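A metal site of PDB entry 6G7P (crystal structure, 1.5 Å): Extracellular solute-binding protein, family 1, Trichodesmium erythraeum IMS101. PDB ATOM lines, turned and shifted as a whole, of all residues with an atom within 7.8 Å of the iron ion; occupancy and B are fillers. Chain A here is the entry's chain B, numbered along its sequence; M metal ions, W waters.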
ATOM      1  N   ARG A   9     -32.737  15.806 -12.393  1.00  0.00           N
ATOM      2  CA  ARG A   9     -32.293  17.078 -12.883  1.00  0.00           C
ATOM      3  C   ARG A   9     -32.901  18.266 -12.096  1.00  0.00           C
ATOM      4  O   ARG A   9     -32.708  19.415 -12.422  1.00  0.00           O
ATOM      5  CB  ARG A   9     -32.651  17.107 -14.383  1.00  0.00           C
ATOM      6  CG  ARG A   9     -32.408  18.394 -15.203  1.00  0.00           C
ATOM      7  CD  ARG A   9     -31.011  18.993 -15.110  1.00  0.00           C
ATOM      8  NE  ARG A   9     -30.906  20.188 -15.904  1.00  0.00           N
ATOM      9  CZ  ARG A   9     -31.424  21.389 -15.557  1.00  0.00           C
ATOM     10  NH1 ARG A   9     -31.983  21.573 -14.385  1.00  0.00           N
ATOM     11  NH2 ARG A   9     -31.318  22.437 -16.370  1.00  0.00           N
ATOM     12  N   TYR A  11     -33.258  21.076  -9.445  1.00  0.00           N
ATOM     13  CA  TYR A  11     -32.558  22.001  -8.553  1.00  0.00           C
ATOM     14  C   TYR A  11     -33.609  22.770  -7.759  1.00  0.00           C
ATOM     15  O   TYR A  11     -34.717  22.960  -8.209  1.00  0.00           O
ATOM     16  CB  TYR A  11     -31.631  22.939  -9.312  1.00  0.00           C
ATOM     17  CG  TYR A  11     -30.466  22.214  -9.893  1.00  0.00           C
ATOM     18  CD1 TYR A  11     -30.525  21.626 -11.157  1.00  0.00           C
ATOM     19  CD2 TYR A  11     -29.284  22.068  -9.169  1.00  0.00           C
ATOM     20  CE1 TYR A  11     -29.438  20.914 -11.677  1.00  0.00           C
ATOM     21  CE2 TYR A  11     -28.204  21.369  -9.699  1.00  0.00           C
ATOM     22  CZ  TYR A  11     -28.291  20.823 -10.961  1.00  0.00           C
ATOM     23  OH  TYR A  11     -27.220  20.126 -11.461  1.00  0.00           O
ATOM     24  N   VAL A  58     -30.613  13.950 -17.543  1.00  0.00           N
ATOM     25  CA  VAL A  58     -29.649  14.633 -18.337  1.00  0.00           C
ATOM     26  C   VAL A  58     -28.971  13.653 -19.292  1.00  0.00           C
ATOM     27  O   VAL A  58     -28.715  12.483 -18.937  1.00  0.00           O
ATOM     28  CB  VAL A  58     -28.609  15.221 -17.342  1.00  0.00           C
ATOM     29  CG1 VAL A  58     -27.283  15.501 -17.917  1.00  0.00           C
ATOM     30  CG2 VAL A  58     -29.205  16.455 -16.713  1.00  0.00           C
ATOM     31  N   ARG A  62     -28.823   9.025 -21.893  1.00  0.00           N
ATOM     32  CA  ARG A  62     -29.681   8.481 -20.832  1.00  0.00           C
ATOM     33  C   ARG A  62     -31.146   8.434 -21.256  1.00  0.00           C
ATOM     34  O   ARG A  62     -31.899   7.501 -20.927  1.00  0.00           O
ATOM     35  CB  ARG A  62     -29.565   9.260 -19.537  1.00  0.00           C
ATOM     36  CG  ARG A  62     -28.260   9.132 -18.773  1.00  0.00           C
ATOM     37  CD  ARG A  62     -28.502   9.420 -17.284  1.00  0.00           C
ATOM     38  NE  ARG A  62     -27.286   9.462 -16.521  1.00  0.00           N
ATOM     39  CZ  ARG A  62     -26.515  10.538 -16.310  1.00  0.00           C
ATOM     40  NH1 ARG A  62     -25.395  10.488 -15.582  1.00  0.00           N
ATOM     41  NH2 ARG A  62     -26.862  11.695 -16.797  1.00  0.00           N
ATOM     42  N   ARG A 101     -26.601  21.912 -23.229  1.00  0.00           N
ATOM     43  CA  ARG A 101     -25.204  22.067 -22.780  1.00  0.00           C
ATOM     44  C   ARG A 101     -24.307  21.819 -23.955  1.00  0.00           C
ATOM     45  O   ARG A 101     -24.675  21.152 -24.914  1.00  0.00           O
ATOM     46  CB  ARG A 101     -24.884  21.158 -21.609  1.00  0.00           C
ATOM     47  CG  ARG A 101     -25.096  19.622 -21.854  1.00  0.00           C
ATOM     48  CD  ARG A 101     -26.495  19.052 -21.486  1.00  0.00           C
ATOM     49  NE  ARG A 101     -26.833  19.281 -20.051  1.00  0.00           N
ATOM     50  CZ  ARG A 101     -26.335  18.616 -19.046  1.00  0.00           C
ATOM     51  NH1 ARG A 101     -26.704  18.919 -17.797  1.00  0.00           N
ATOM     52  NH2 ARG A 101     -25.492  17.641 -19.220  1.00  0.00           N
ATOM     53  N   ARG A 103     -20.328  20.379 -25.006  1.00  0.00           N
ATOM     54  CA  ARG A 103     -19.097  19.689 -24.524  1.00  0.00           C
ATOM     55  C   ARG A 103     -17.943  20.366 -25.257  1.00  0.00           C
ATOM     56  O   ARG A 103     -17.785  20.250 -26.466  1.00  0.00           O
ATOM     57  CB  ARG A 103     -19.154  18.168 -24.669  1.00  0.00           C
ATOM     58  CG  ARG A 103     -18.103  17.489 -23.835  1.00  0.00           C
ATOM     59  CD  ARG A 103     -18.537  16.098 -23.372  1.00  0.00           C
ATOM     60  NE  ARG A 103     -17.666  15.474 -22.405  1.00  0.00           N
ATOM     61  CZ  ARG A 103     -17.587  15.841 -21.112  1.00  0.00           C
ATOM     62  NH1 ARG A 103     -18.387  16.774 -20.650  1.00  0.00           N
ATOM     63  NH2 ARG A 103     -16.773  15.214 -20.286  1.00  0.00           N
ATOM     64  N   ARG A 135     -12.257  13.123 -17.958  1.00  0.00           N
ATOM     65  CA  ARG A 135     -12.752  12.078 -17.044  1.00  0.00           C
ATOM     66  C   ARG A 135     -12.907  10.728 -17.730  1.00  0.00           C
ATOM     67  O   ARG A 135     -12.689  10.570 -18.941  1.00  0.00           O
ATOM     68  CB  ARG A 135     -14.035  12.523 -16.409  1.00  0.00           C
ATOM     69  CG  ARG A 135     -15.226  12.502 -17.311  1.00  0.00           C
ATOM     70  CD  ARG A 135     -16.427  13.187 -16.733  1.00  0.00           C
ATOM     71  NE  ARG A 135     -16.953  12.612 -15.503  1.00  0.00           N
ATOM     72  CZ  ARG A 135     -17.982  13.115 -14.824  1.00  0.00           C
ATOM     73  NH1 ARG A 135     -18.555  14.260 -15.211  1.00  0.00           N
ATOM     74  NH2 ARG A 135     -18.389  12.497 -13.737  1.00  0.00           N
ATOM     75  N   ASN A 139     -18.392   7.808 -18.104  1.00  0.00           N
ATOM     76  CA  ASN A 139     -19.257   8.999 -18.058  1.00  0.00           C
ATOM     77  C   ASN A 139     -20.065   9.183 -19.330  1.00  0.00           C
ATOM     78  O   ASN A 139     -19.501   9.099 -20.426  1.00  0.00           O
ATOM     79  CB  ASN A 139     -18.408  10.237 -17.808  1.00  0.00           C
ATOM     80  CG  ASN A 139     -19.183  11.548 -18.006  1.00  0.00           C
ATOM     81  OD1 ASN A 139     -18.988  12.194 -19.022  1.00  0.00           O
ATOM     82  ND2 ASN A 139     -19.997  11.898 -17.085  1.00  0.00           N
ATOM     83  N   ILE A 140     -21.365   9.394 -19.148  1.00  0.00           N
ATOM     84  CA  ILE A 140     -22.247   9.480 -20.305  1.00  0.00           C
ATOM     85  C   ILE A 140     -21.892  10.669 -21.210  1.00  0.00           C
ATOM     86  O   ILE A 140     -22.088  10.542 -22.459  1.00  0.00           O
ATOM     87  CB  ILE A 140     -23.720   9.546 -19.851  1.00  0.00           C
ATOM     88  CG1 ILE A 140     -24.682   9.310 -21.006  1.00  0.00           C
ATOM     89  CG2 ILE A 140     -24.058  10.845 -19.157  1.00  0.00           C
ATOM     90  CD1 ILE A 140     -24.673   7.937 -21.553  1.00  0.00           C
ATOM     91  N   TYR A 141     -21.389  11.779 -20.688  1.00  0.00           N
ATOM     92  CA  TYR A 141     -21.102  12.895 -21.567  1.00  0.00           C
ATOM     93  C   TYR A 141     -20.014  12.517 -22.569  1.00  0.00           C
ATOM     94  O   TYR A 141     -20.073  12.869 -23.752  1.00  0.00           O
ATOM     95  CB  TYR A 141     -20.629  14.118 -20.788  1.00  0.00           C
ATOM     96  CG  TYR A 141     -21.441  14.516 -19.584  1.00  0.00           C
ATOM     97  CD1 TYR A 141     -22.819  14.391 -19.551  1.00  0.00           C
ATOM     98  CD2 TYR A 141     -20.804  15.035 -18.443  1.00  0.00           C
ATOM     99  CE1 TYR A 141     -23.527  14.820 -18.425  1.00  0.00           C
ATOM    100  CE2 TYR A 141     -21.509  15.444 -17.359  1.00  0.00           C
ATOM    101  CZ  TYR A 141     -22.889  15.342 -17.335  1.00  0.00           C
ATOM    102  OH  TYR A 141     -23.607  15.744 -16.221  1.00  0.00           O
ATOM    103  N   ASP A 177     -16.161  16.423 -14.229  1.00  0.00           N
ATOM    104  CA  ASP A 177     -15.814  17.500 -15.171  1.00  0.00           C
ATOM    105  C   ASP A 177     -15.193  18.696 -14.443  1.00  0.00           C
ATOM    106  O   ASP A 177     -14.232  19.322 -14.959  1.00  0.00           O
ATOM    107  CB  ASP A 177     -17.057  17.990 -15.965  1.00  0.00           C
ATOM    108  CG  ASP A 177     -17.325  17.232 -17.249  1.00  0.00           C
ATOM    109  OD1 ASP A 177     -16.736  16.169 -17.488  1.00  0.00           O
ATOM    110  OD2 ASP A 177     -18.162  17.759 -18.031  1.00  0.00           O
ATOM    111  N   ASN A 195     -18.388  19.975 -19.831  1.00  0.00           N
ATOM    112  CA  ASN A 195     -19.583  20.670 -20.223  1.00  0.00           C
ATOM    113  C   ASN A 195     -19.468  22.135 -19.831  1.00  0.00           C
ATOM    114  O   ASN A 195     -18.990  22.503 -18.769  1.00  0.00           O
ATOM    115  CB  ASN A 195     -20.854  20.032 -19.648  1.00  0.00           C
ATOM    116  CG  ASN A 195     -21.180  18.673 -20.244  1.00  0.00           C
ATOM    117  OD1 ASN A 195     -20.702  18.344 -21.344  1.00  0.00           O
ATOM    118  ND2 ASN A 195     -22.013  17.917 -19.545  1.00  0.00           N
ATOM    119  N   TYR A 197     -21.586  24.350 -18.686  1.00  0.00           N
ATOM    120  CA  TYR A 197     -22.166  24.865 -17.436  1.00  0.00           C
ATOM    121  C   TYR A 197     -21.273  24.687 -16.214  1.00  0.00           C
ATOM    122  O   TYR A 197     -21.462  25.366 -15.235  1.00  0.00           O
ATOM    123  CB  TYR A 197     -23.560  24.258 -17.209  1.00  0.00           C
ATOM    124  CG  TYR A 197     -23.581  22.764 -17.112  1.00  0.00           C
ATOM    125  CD1 TYR A 197     -23.321  22.110 -15.947  1.00  0.00           C
ATOM    126  CD2 TYR A 197     -23.846  21.976 -18.238  1.00  0.00           C
ATOM    127  CE1 TYR A 197     -23.369  20.723 -15.894  1.00  0.00           C
ATOM    128  CE2 TYR A 197     -23.815  20.605 -18.214  1.00  0.00           C
ATOM    129  CZ  TYR A 197     -23.560  19.962 -17.018  1.00  0.00           C
ATOM    130  OH  TYR A 197     -23.504  18.602 -16.963  1.00  0.00           O
ATOM    131  N   TYR A 198     -20.315  23.760 -16.255  1.00  0.00           N
ATOM    132  CA  TYR A 198     -19.415  23.603 -15.082  1.00  0.00           C
ATOM    133  C   TYR A 198     -18.478  24.795 -14.955  1.00  0.00           C
ATOM    134  O   TYR A 198     -18.093  25.139 -13.835  1.00  0.00           O
ATOM    135  CB  TYR A 198     -18.624  22.293 -15.195  1.00  0.00           C
ATOM    136  CG  TYR A 198     -19.464  21.058 -14.993  1.00  0.00           C
ATOM    137  CD1 TYR A 198     -20.115  20.796 -13.816  1.00  0.00           C
ATOM    138  CD2 TYR A 198     -19.664  20.146 -16.025  1.00  0.00           C
ATOM    139  CE1 TYR A 198     -20.884  19.678 -13.678  1.00  0.00           C
ATOM    140  CE2 TYR A 198     -20.429  19.037 -15.887  1.00  0.00           C
ATOM    141  CZ  TYR A 198     -21.026  18.808 -14.688  1.00  0.00           C
ATOM    142  OH  TYR A 198     -21.845  17.728 -14.538  1.00  0.00           O
ATOM    143  N   ARG A 201     -20.674  27.532 -13.542  1.00  0.00           N
ATOM    144  CA  ARG A 201     -20.924  27.255 -12.135  1.00  0.00           C
ATOM    145  C   ARG A 201     -19.805  27.833 -11.261  1.00  0.00           C
ATOM    146  O   ARG A 201     -20.066  28.513 -10.212  1.00  0.00           O
ATOM    147  CB  ARG A 201     -21.093  25.753 -11.908  1.00  0.00           C
ATOM    148  CG  ARG A 201     -21.575  25.390 -10.566  1.00  0.00           C
ATOM    149  CD  ARG A 201     -21.704  23.887 -10.379  1.00  0.00           C
ATOM    150  NE  ARG A 201     -22.685  23.249 -11.256  1.00  0.00           N
ATOM    151  CZ  ARG A 201     -22.880  21.931 -11.309  1.00  0.00           C
ATOM    152  NH1 ARG A 201     -22.152  21.093 -10.555  1.00  0.00           N
ATOM    153  NH2 ARG A 201     -23.821  21.432 -12.058  1.00  0.00           N
ATOM    154  N   SER A 234     -30.558  18.482 -21.358  1.00  0.00           N
ATOM    155  CA  SER A 234     -31.395  18.053 -20.220  1.00  0.00           C
ATOM    156  C   SER A 234     -32.793  17.875 -20.811  1.00  0.00           C
ATOM    157  O   SER A 234     -33.274  18.779 -21.462  1.00  0.00           O
ATOM    158  CB  SER A 234     -31.461  19.142 -19.158  1.00  0.00           C
ATOM    159  OG  SER A 234     -30.183  19.373 -18.574  1.00  0.00           O
ATOM    160  N   ASN A 268     -29.284  25.429 -13.910  1.00  0.00           N
ATOM    161  CA  ASN A 268     -28.007  24.756 -14.027  1.00  0.00           C
ATOM    162  C   ASN A 268     -27.074  25.450 -15.020  1.00  0.00           C
ATOM    163  O   ASN A 268     -26.188  24.831 -15.555  1.00  0.00           O
ATOM    164  CB  ASN A 268     -28.176  23.289 -14.440  1.00  0.00           C
ATOM    165  CG  ASN A 268     -26.903  22.494 -14.243  1.00  0.00           C
ATOM    166  OD1 ASN A 268     -26.141  22.715 -13.289  1.00  0.00           O
ATOM    167  ND2 ASN A 268     -26.626  21.578 -15.156  1.00  0.00           N
ATOM    168  N   GLU A 270     -27.367  26.355 -18.005  1.00  0.00           N
ATOM    169  CA  GLU A 270     -27.499  25.807 -19.327  1.00  0.00           C
ATOM    170  C   GLU A 270     -28.136  26.823 -20.232  1.00  0.00           C
ATOM    171  O   GLU A 270     -28.599  27.873 -19.803  1.00  0.00           O
ATOM    172  CB  GLU A 270     -28.289  24.479 -19.281  1.00  0.00           C
ATOM    173  CG  GLU A 270     -27.507  23.371 -18.581  1.00  0.00           C
ATOM    174  CD  GLU A 270     -28.187  22.028 -18.576  1.00  0.00           C
ATOM    175  OE1 GLU A 270     -28.697  21.596 -19.622  1.00  0.00           O
ATOM    176  OE2 GLU A 270     -28.174  21.402 -17.519  1.00  0.00           O
HETATM  177 FE    FE M   1     -23.646  17.438 -15.355  1.00  0.00          FE
HETATM  178  O   HOH W   1     -24.200  18.658 -13.395  1.00  0.00           O
HETATM  179  O   HOH W   2     -25.653  17.938 -15.338  1.00  0.00           O
HETATM  180  O   HOH W   3     -24.251  16.394 -13.571  1.00  0.00           O
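OH of Tyr 197 sits close to ND2 of Asn 195. The side-chain amide oxygen (OD1) of Asn 139 lies within hydrogen-bond range of the backbone NH (N) of Tyr 141 (3.0 Å). The side-chain hydroxyl of Tyr 197 lies close to the guanidinium group of Arg 101 (3.2 Å).
The side-chain hydroxyl (OH) of Tyr 141 binds the iron ion (1.9 Å). The iron ion is bound by the side-chain hydroxyl (OH) of Tyr 197, at 2.0 Å. OH of Tyr 198 is bound to the iron ion (2.0 Å). Water W2 binds the iron ion (2.1 Å). Water W3 is bound to the iron ion. The iron ion is bound by water W1, 2.4 Å away.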
